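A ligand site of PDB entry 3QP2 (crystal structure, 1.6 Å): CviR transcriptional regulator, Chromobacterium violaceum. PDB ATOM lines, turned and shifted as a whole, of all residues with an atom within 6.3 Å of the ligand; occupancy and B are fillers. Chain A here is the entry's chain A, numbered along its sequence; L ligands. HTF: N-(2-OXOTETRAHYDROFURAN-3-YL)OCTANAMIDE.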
ATOM      1  N   LEU A  52     -17.784 -12.544 -27.683  1.00  0.00           N
ATOM      2  CA  LEU A  52     -16.759 -11.752 -26.989  1.00  0.00           C
ATOM      3  C   LEU A  52     -15.392 -12.364 -27.271  1.00  0.00           C
ATOM      4  O   LEU A  52     -15.241 -13.588 -27.327  1.00  0.00           O
ATOM      5  CB  LEU A  52     -17.028 -11.711 -25.469  1.00  0.00           C
ATOM      6  CG  LEU A  52     -16.027 -10.917 -24.617  1.00  0.00           C
ATOM      7  CD1 LEU A  52     -16.727 -10.175 -23.455  1.00  0.00           C
ATOM      8  CD2 LEU A  52     -14.920 -11.828 -24.102  1.00  0.00           C
ATOM      9  N   ALA A  54     -11.288 -12.167 -25.956  1.00  0.00           N
ATOM     10  CA  ALA A  54     -10.379 -11.623 -24.944  1.00  0.00           C
ATOM     11  C   ALA A  54      -8.964 -12.138 -25.128  1.00  0.00           C
ATOM     12  O   ALA A  54      -8.740 -13.264 -25.572  1.00  0.00           O
ATOM     13  CB  ALA A  54     -10.898 -11.926 -23.547  1.00  0.00           C
ATOM     14  N   LEU A  67      -6.094 -10.675 -17.675  1.00  0.00           N
ATOM     15  CA  LEU A  67      -6.765 -10.258 -18.901  1.00  0.00           C
ATOM     16  C   LEU A  67      -6.155  -8.960 -19.414  1.00  0.00           C
ATOM     17  O   LEU A  67      -6.092  -7.971 -18.683  1.00  0.00           O
ATOM     18  CB  LEU A  67      -8.262 -10.063 -18.655  1.00  0.00           C
ATOM     19  CG  LEU A  67      -9.100 -11.320 -18.464  1.00  0.00           C
ATOM     20  CD1 LEU A  67     -10.422 -10.962 -17.816  1.00  0.00           C
ATOM     21  CD2 LEU A  67      -9.314 -12.018 -19.798  1.00  0.00           C
ATOM     22  N   VAL A  70     -10.205  -6.920 -23.571  1.00  0.00           N
ATOM     23  CA  VAL A  70     -11.494  -7.555 -23.778  1.00  0.00           C
ATOM     24  C   VAL A  70     -12.170  -6.814 -24.900  1.00  0.00           C
ATOM     25  O   VAL A  70     -12.341  -5.588 -24.825  1.00  0.00           O
ATOM     26  CB  VAL A  70     -12.387  -7.516 -22.522  1.00  0.00           C
ATOM     27  CG1 VAL A  70     -13.760  -8.132 -22.819  1.00  0.00           C
ATOM     28  CG2 VAL A  70     -11.718  -8.217 -21.348  1.00  0.00           C
ATOM     29  N   TYR A  75     -21.960  -9.320 -26.094  1.00  0.00           N
ATOM     30  CA  TYR A  75     -22.428  -9.626 -24.746  1.00  0.00           C
ATOM     31  C   TYR A  75     -23.230  -8.427 -24.256  1.00  0.00           C
ATOM     32  O   TYR A  75     -22.847  -7.281 -24.519  1.00  0.00           O
ATOM     33  CB  TYR A  75     -21.258  -9.855 -23.785  1.00  0.00           C
ATOM     34  CG  TYR A  75     -20.698 -11.262 -23.751  1.00  0.00           C
ATOM     35  CD1 TYR A  75     -20.030 -11.720 -22.620  1.00  0.00           C
ATOM     36  CD2 TYR A  75     -20.821 -12.118 -24.838  1.00  0.00           C
ATOM     37  CE1 TYR A  75     -19.518 -12.998 -22.559  1.00  0.00           C
ATOM     38  CE2 TYR A  75     -20.296 -13.408 -24.795  1.00  0.00           C
ATOM     39  CZ  TYR A  75     -19.640 -13.836 -23.646  1.00  0.00           C
ATOM     40  OH  TYR A  75     -19.110 -15.098 -23.568  1.00  0.00           O
ATOM     41  N   TRP A  79     -24.563  -7.453 -18.271  1.00  0.00           N
ATOM     42  CA  TRP A  79     -23.893  -8.671 -17.812  1.00  0.00           C
ATOM     43  C   TRP A  79     -22.397  -8.407 -17.576  1.00  0.00           C
ATOM     44  O   TRP A  79     -21.830  -8.856 -16.572  1.00  0.00           O
ATOM     45  CB  TRP A  79     -24.097  -9.824 -18.807  1.00  0.00           C
ATOM     46  CG  TRP A  79     -23.284 -11.065 -18.485  1.00  0.00           C
ATOM     47  CD1 TRP A  79     -22.306 -11.637 -19.269  1.00  0.00           C
ATOM     48  CD2 TRP A  79     -23.367 -11.854 -17.297  1.00  0.00           C
ATOM     49  NE1 TRP A  79     -21.781 -12.733 -18.629  1.00  0.00           N
ATOM     50  CE2 TRP A  79     -22.422 -12.900 -17.427  1.00  0.00           C
ATOM     51  CE3 TRP A  79     -24.157 -11.802 -16.138  1.00  0.00           C
ATOM     52  CZ2 TRP A  79     -22.226 -13.867 -16.431  1.00  0.00           C
ATOM     53  CZ3 TRP A  79     -23.967 -12.757 -15.148  1.00  0.00           C
ATOM     54  CH2 TRP A  79     -23.007 -13.781 -15.296  1.00  0.00           C
ATOM     55  N   LEU A  80     -21.768  -7.701 -18.496  1.00  0.00           N
ATOM     56  CA  LEU A  80     -20.348  -7.383 -18.372  1.00  0.00           C
ATOM     57  C   LEU A  80     -20.082  -6.497 -17.167  1.00  0.00           C
ATOM     58  O   LEU A  80     -19.131  -6.707 -16.416  1.00  0.00           O
ATOM     59  CB  LEU A  80     -19.841  -6.708 -19.634  1.00  0.00           C
ATOM     60  CG  LEU A  80     -19.758  -7.607 -20.851  1.00  0.00           C
ATOM     61  CD1 LEU A  80     -19.143  -6.832 -21.993  1.00  0.00           C
ATOM     62  CD2 LEU A  80     -18.933  -8.838 -20.517  1.00  0.00           C
ATOM     63  N   TYR A  83     -20.364  -8.765 -14.155  1.00  0.00           N
ATOM     64  CA  TYR A  83     -19.205  -9.651 -14.140  1.00  0.00           C
ATOM     65  C   TYR A  83     -17.996  -8.947 -13.527  1.00  0.00           C
ATOM     66  O   TYR A  83     -17.279  -9.512 -12.699  1.00  0.00           O
ATOM     67  CB  TYR A  83     -18.918 -10.056 -15.586  1.00  0.00           C
ATOM     68  CG  TYR A  83     -17.984 -11.217 -15.765  1.00  0.00           C
ATOM     69  CD1 TYR A  83     -18.455 -12.473 -16.143  1.00  0.00           C
ATOM     70  CD2 TYR A  83     -16.615 -11.070 -15.564  1.00  0.00           C
ATOM     71  CE1 TYR A  83     -17.601 -13.540 -16.318  1.00  0.00           C
ATOM     72  CE2 TYR A  83     -15.756 -12.119 -15.725  1.00  0.00           C
ATOM     73  CZ  TYR A  83     -16.248 -13.351 -16.105  1.00  0.00           C
ATOM     74  OH  TYR A  83     -15.373 -14.395 -16.270  1.00  0.00           O
ATOM     75  N   MET A  84     -17.772  -7.709 -13.940  1.00  0.00           N
ATOM     76  CA  MET A  84     -16.660  -6.921 -13.413  1.00  0.00           C
ATOM     77  C   MET A  84     -16.919  -6.477 -11.981  1.00  0.00           C
ATOM     78  O   MET A  84     -16.056  -6.585 -11.121  1.00  0.00           O
ATOM     79  CB  MET A  84     -16.382  -5.711 -14.312  1.00  0.00           C
ATOM     80  CG  MET A  84     -15.825  -6.097 -15.670  1.00  0.00           C
ATOM     81  SD  MET A  84     -14.295  -7.030 -15.520  1.00  0.00           S
ATOM     82  CE  MET A  84     -13.185  -5.762 -14.902  1.00  0.00           C
ATOM     83  N   ASP A  92     -15.514 -17.913 -12.634  1.00  0.00           N
ATOM     84  CA  ASP A  92     -16.034 -18.369 -13.929  1.00  0.00           C
ATOM     85  C   ASP A  92     -15.184 -19.523 -14.422  1.00  0.00           C
ATOM     86  O   ASP A  92     -14.010 -19.337 -14.727  1.00  0.00           O
ATOM     87  CB  ASP A  92     -15.987 -17.208 -14.925  1.00  0.00           C
ATOM     88  CG  ASP A  92     -16.442 -17.597 -16.330  1.00  0.00           C
ATOM     89  OD1 ASP A  92     -16.769 -18.782 -16.561  1.00  0.00           O
ATOM     90  OD2 ASP A  92     -16.489 -16.699 -17.188  1.00  0.00           O
ATOM     91  N   PRO A  93     -15.761 -20.739 -14.462  1.00  0.00           N
ATOM     92  CA  PRO A  93     -15.020 -21.929 -14.915  1.00  0.00           C
ATOM     93  C   PRO A  93     -14.403 -21.734 -16.307  1.00  0.00           C
ATOM     94  O   PRO A  93     -13.377 -22.345 -16.608  1.00  0.00           O
ATOM     95  CB  PRO A  93     -16.101 -23.011 -14.956  1.00  0.00           C
ATOM     96  CG  PRO A  93     -17.135 -22.558 -13.970  1.00  0.00           C
ATOM     97  CD  PRO A  93     -17.161 -21.067 -14.103  1.00  0.00           C
ATOM     98  N   ILE A  94     -15.013 -20.883 -17.138  1.00  0.00           N
ATOM     99  CA  ILE A  94     -14.489 -20.638 -18.486  1.00  0.00           C
ATOM    100  C   ILE A  94     -13.108 -19.960 -18.461  1.00  0.00           C
ATOM    101  O   ILE A  94     -12.270 -20.221 -19.334  1.00  0.00           O
ATOM    102  CB  ILE A  94     -15.483 -19.837 -19.349  1.00  0.00           C
ATOM    103  CG1 ILE A  94     -16.852 -20.527 -19.392  1.00  0.00           C
ATOM    104  CG2 ILE A  94     -14.917 -19.617 -20.765  1.00  0.00           C
ATOM    105  CD1 ILE A  94     -16.789 -22.004 -19.682  1.00  0.00           C
ATOM    106  N   LEU A  95     -12.848 -19.116 -17.465  1.00  0.00           N
ATOM    107  CA  LEU A  95     -11.531 -18.488 -17.381  1.00  0.00           C
ATOM    108  C   LEU A  95     -10.455 -19.414 -16.837  1.00  0.00           C
ATOM    109  O   LEU A  95      -9.284 -19.035 -16.762  1.00  0.00           O
ATOM    110  CB  LEU A  95     -11.568 -17.165 -16.596  1.00  0.00           C
ATOM    111  CG  LEU A  95     -12.314 -15.997 -17.255  1.00  0.00           C
ATOM    112  CD1 LEU A  95     -12.009 -14.705 -16.509  1.00  0.00           C
ATOM    113  CD2 LEU A  95     -11.931 -15.857 -18.737  1.00  0.00           C
ATOM    114  N   TRP A 106     -19.879 -25.042 -22.599  1.00  0.00           N
ATOM    115  CA  TRP A 106     -20.087 -24.508 -21.252  1.00  0.00           C
ATOM    116  C   TRP A 106     -20.937 -25.431 -20.381  1.00  0.00           C
ATOM    117  O   TRP A 106     -20.635 -25.627 -19.203  1.00  0.00           O
ATOM    118  CB  TRP A 106     -20.745 -23.126 -21.284  1.00  0.00           C
ATOM    119  CG  TRP A 106     -19.968 -22.043 -21.962  1.00  0.00           C
ATOM    120  CD1 TRP A 106     -18.717 -22.132 -22.490  1.00  0.00           C
ATOM    121  CD2 TRP A 106     -20.403 -20.699 -22.179  1.00  0.00           C
ATOM    122  NE1 TRP A 106     -18.352 -20.923 -23.032  1.00  0.00           N
ATOM    123  CE2 TRP A 106     -19.376 -20.024 -22.854  1.00  0.00           C
ATOM    124  CE3 TRP A 106     -21.589 -20.013 -21.875  1.00  0.00           C
ATOM    125  CZ2 TRP A 106     -19.480 -18.676 -23.216  1.00  0.00           C
ATOM    126  CZ3 TRP A 106     -21.696 -18.670 -22.230  1.00  0.00           C
ATOM    127  CH2 TRP A 106     -20.654 -18.024 -22.908  1.00  0.00           C
ATOM    128  N   PHE A 110     -19.884 -26.562 -16.835  1.00  0.00           N
ATOM    129  CA  PHE A 110     -20.656 -26.088 -15.686  1.00  0.00           C
ATOM    130  C   PHE A 110     -21.189 -27.243 -14.842  1.00  0.00           C
ATOM    131  O   PHE A 110     -21.227 -27.166 -13.603  1.00  0.00           O
ATOM    132  CB  PHE A 110     -21.815 -25.187 -16.123  1.00  0.00           C
ATOM    133  CG  PHE A 110     -21.379 -23.854 -16.667  1.00  0.00           C
ATOM    134  CD1 PHE A 110     -20.064 -23.428 -16.525  1.00  0.00           C
ATOM    135  CD2 PHE A 110     -22.281 -23.021 -17.311  1.00  0.00           C
ATOM    136  CE1 PHE A 110     -19.662 -22.203 -17.017  1.00  0.00           C
ATOM    137  CE2 PHE A 110     -21.884 -21.784 -17.810  1.00  0.00           C
ATOM    138  CZ  PHE A 110     -20.572 -21.381 -17.660  1.00  0.00           C
ATOM    139  N   PHE A 121     -22.025 -18.450  -9.404  1.00  0.00           N
ATOM    140  CA  PHE A 121     -21.770 -17.807 -10.693  1.00  0.00           C
ATOM    141  C   PHE A 121     -22.593 -18.458 -11.806  1.00  0.00           C
ATOM    142  O   PHE A 121     -23.220 -17.781 -12.627  1.00  0.00           O
ATOM    143  CB  PHE A 121     -20.294 -17.869 -11.079  1.00  0.00           C
ATOM    144  CG  PHE A 121     -20.041 -17.527 -12.521  1.00  0.00           C
ATOM    145  CD1 PHE A 121     -19.996 -16.202 -12.941  1.00  0.00           C
ATOM    146  CD2 PHE A 121     -19.881 -18.532 -13.458  1.00  0.00           C
ATOM    147  CE1 PHE A 121     -19.782 -15.893 -14.279  1.00  0.00           C
ATOM    148  CE2 PHE A 121     -19.676 -18.228 -14.816  1.00  0.00           C
ATOM    149  CZ  PHE A 121     -19.636 -16.914 -15.221  1.00  0.00           C
ATOM    150  N   ALA A 125     -25.151 -16.666 -14.200  1.00  0.00           N
ATOM    151  CA  ALA A 125     -24.958 -16.692 -15.658  1.00  0.00           C
ATOM    152  C   ALA A 125     -26.171 -17.258 -16.364  1.00  0.00           C
ATOM    153  O   ALA A 125     -26.627 -16.715 -17.379  1.00  0.00           O
ATOM    154  CB  ALA A 125     -23.703 -17.485 -16.030  1.00  0.00           C
ATOM    155  N   MET A 130     -26.700 -16.813 -20.170  1.00  0.00           N
ATOM    156  CA  MET A 130     -25.321 -17.205 -20.417  1.00  0.00           C
ATOM    157  C   MET A 130     -25.003 -18.607 -19.910  1.00  0.00           C
ATOM    158  O   MET A 130     -23.846 -18.913 -19.594  1.00  0.00           O
ATOM    159  CB  MET A 130     -24.360 -16.215 -19.729  1.00  0.00           C
ATOM    160  CG  MET A 130     -24.489 -14.768 -20.194  1.00  0.00           C
ATOM    161  SD  MET A 130     -24.331 -14.713 -22.000  1.00  0.00           S
ATOM    162  CE  MET A 130     -24.045 -12.975 -22.288  1.00  0.00           C
ATOM    163  N   GLY A 131     -26.021 -19.453 -19.813  1.00  0.00           N
ATOM    164  CA  GLY A 131     -25.850 -20.779 -19.248  1.00  0.00           C
ATOM    165  C   GLY A 131     -25.302 -21.787 -20.229  1.00  0.00           C
ATOM    166  O   GLY A 131     -24.773 -22.832 -19.844  1.00  0.00           O
ATOM    167  N   THR A 135     -16.507 -21.901 -25.904  1.00  0.00           N
ATOM    168  CA  THR A 135     -15.315 -21.049 -25.941  1.00  0.00           C
ATOM    169  C   THR A 135     -14.186 -21.724 -26.726  1.00  0.00           C
ATOM    170  O   THR A 135     -13.792 -22.852 -26.418  1.00  0.00           O
ATOM    171  CB  THR A 135     -14.835 -20.649 -24.521  1.00  0.00           C
ATOM    172  OG1 THR A 135     -15.857 -19.858 -23.885  1.00  0.00           O
ATOM    173  CG2 THR A 135     -13.553 -19.813 -24.616  1.00  0.00           C
ATOM    174  N   ILE A 148      -9.226 -16.103 -26.113  1.00  0.00           N
ATOM    175  CA  ILE A 148     -10.445 -16.890 -26.076  1.00  0.00           C
ATOM    176  C   ILE A 148     -11.503 -16.191 -26.930  1.00  0.00           C
ATOM    177  O   ILE A 148     -11.603 -14.962 -26.945  1.00  0.00           O
ATOM    178  CB  ILE A 148     -10.979 -17.094 -24.638  1.00  0.00           C
ATOM    179  CG1 ILE A 148     -11.120 -15.756 -23.901  1.00  0.00           C
ATOM    180  CG2 ILE A 148     -10.086 -18.047 -23.854  1.00  0.00           C
ATOM    181  CD1 ILE A 148     -11.992 -15.891 -22.636  1.00  0.00           C
ATOM    182  N   SER A 150     -15.545 -16.448 -27.264  1.00  0.00           N
ATOM    183  CA  SER A 150     -16.719 -17.026 -26.605  1.00  0.00           C
ATOM    184  C   SER A 150     -17.964 -16.661 -27.365  1.00  0.00           C
ATOM    185  O   SER A 150     -18.144 -15.512 -27.768  1.00  0.00           O
ATOM    186  CB  SER A 150     -16.862 -16.482 -25.179  1.00  0.00           C
ATOM    187  OG  SER A 150     -15.976 -17.134 -24.282  1.00  0.00           O
ATOM    188  N   ILE A 151     -18.829 -17.652 -27.552  1.00  0.00           N
ATOM    189  CA  ILE A 151     -20.117 -17.429 -28.186  1.00  0.00           C
ATOM    190  C   ILE A 151     -21.173 -18.074 -27.308  1.00  0.00           C
ATOM    191  O   ILE A 151     -21.098 -19.259 -27.003  1.00  0.00           O
ATOM    192  CB  ILE A 151     -20.158 -18.024 -29.619  1.00  0.00           C
ATOM    193  CG1 ILE A 151     -19.054 -17.364 -30.458  1.00  0.00           C
ATOM    194  CG2 ILE A 151     -21.530 -17.821 -30.269  1.00  0.00           C
ATOM    195  CD1 ILE A 151     -18.856 -17.956 -31.824  1.00  0.00           C
HETATM  196  C8  HTF L   1     -15.147  -8.828 -18.521  1.00  0.00           C
HETATM  197  C7  HTF L   1     -14.515 -10.056 -19.137  1.00  0.00           C
HETATM  198  C6  HTF L   1     -15.484 -11.222 -19.191  1.00  0.00           C
HETATM  199  C5  HTF L   1     -14.808 -12.383 -19.898  1.00  0.00           C
HETATM  200  C4  HTF L   1     -15.625 -13.659 -19.880  1.00  0.00           C
HETATM  201  C3  HTF L   1     -14.850 -14.650 -20.726  1.00  0.00           C
HETATM  202  C2  HTF L   1     -15.304 -16.077 -20.483  1.00  0.00           C
HETATM  203  C1  HTF L   1     -16.765 -16.239 -20.800  1.00  0.00           C
HETATM  204  O1  HTF L   1     -17.200 -16.078 -21.931  1.00  0.00           O
HETATM  205  N   HTF L   1     -17.513 -16.593 -19.755  1.00  0.00           N
HETATM  206  CA  HTF L   1     -18.924 -16.866 -19.932  1.00  0.00           C
HETATM  207  C   HTF L   1     -19.792 -15.791 -19.361  1.00  0.00           C
HETATM  208  O   HTF L   1     -19.590 -14.591 -19.427  1.00  0.00           O
HETATM  209  OD  HTF L   1     -20.903 -16.382 -18.666  1.00  0.00           O
HETATM  210  CG  HTF L   1     -20.853 -17.806 -18.757  1.00  0.00           C
HETATM  211  CB  HTF L   1     -19.392 -18.087 -19.140  1.00  0.00           C
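CE2 of Tyr 83 touches C6 of the ligand, 3.6 Å away. Met 84 touches the ligand (SD to C8, 3.6 Å). Ile 94 touches the ligand (CG1 to CB, 3.5 Å). CD2 of Leu 95 touches C3 of the ligand, at 3.7 Å. Trp 106 touches the ligand. Phe 110 touches the ligand. Phe 121 touches the ligand. CB of Ala 125 touches CG of the ligand, at 3.96 Å. O of Met 130 touches CG of the ligand, at 3.3 Å. Ile 148 touches the ligand (CD1 to C3, 3.7 Å). Hydrophobic or aromatic side chains within 4 Å of the ligand: Tyr 75, Trp 79, Tyr 83, Met 84, Ile 94, Leu 95, Trp 106, Phe 110, Phe 121, Ala 125, Met 130 and Ile 148. Of the 23 residues printed, 14 come within 4 Å of the ligand. The nearest printed residue that does not touch the ligand is Val 70 (4.01 Å).
The side-chain carboxylate (OD1) of Asp 92 sits at hydrogen-bond distance from the backbone NH (N) of Ile 94, 2.8 Å away. The side-chain carboxylate (OD2) of Asp 92 sits at hydrogen-bond distance from the side-chain hydroxyl (OH) of Tyr 83 (2.7 Å). The backbone carbonyl oxygen (O) of Leu 52 lies within hydrogen-bond range of the backbone NH (N) of Ser 150, at 2.9 Å. OG of Ser 150 sits at hydrogen-bond distance from OG1 of Thr 135 (2.8 Å). The backbone NH (N) of Met 130 is in hydrogen-bond range of the backbone carbonyl oxygen (O) of Ala 125. The indole nitrogen (NE1) of Trp 106 sits at hydrogen-bond distance from the side-chain hydroxyl (OG1) of Thr 135, at 2.8 Å. O of Ala 54 sits at hydrogen-bond distance from N of Ile 148, 2.9 Å away.
O1 of the ligand lies within hydrogen-bond range of OH of Tyr 75, 2.7 Å away. N of the ligand is in hydrogen-bond range of OD2 of Asp 92 (2.8 Å). The side-chain hydroxyl of Ser 150 lies within hydrogen-bond range of an oxygen (O1) of the ligand (2.9 Å). NE1 of Trp 79 is in hydrogen-bond range of O of the ligand (3.0 Å).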
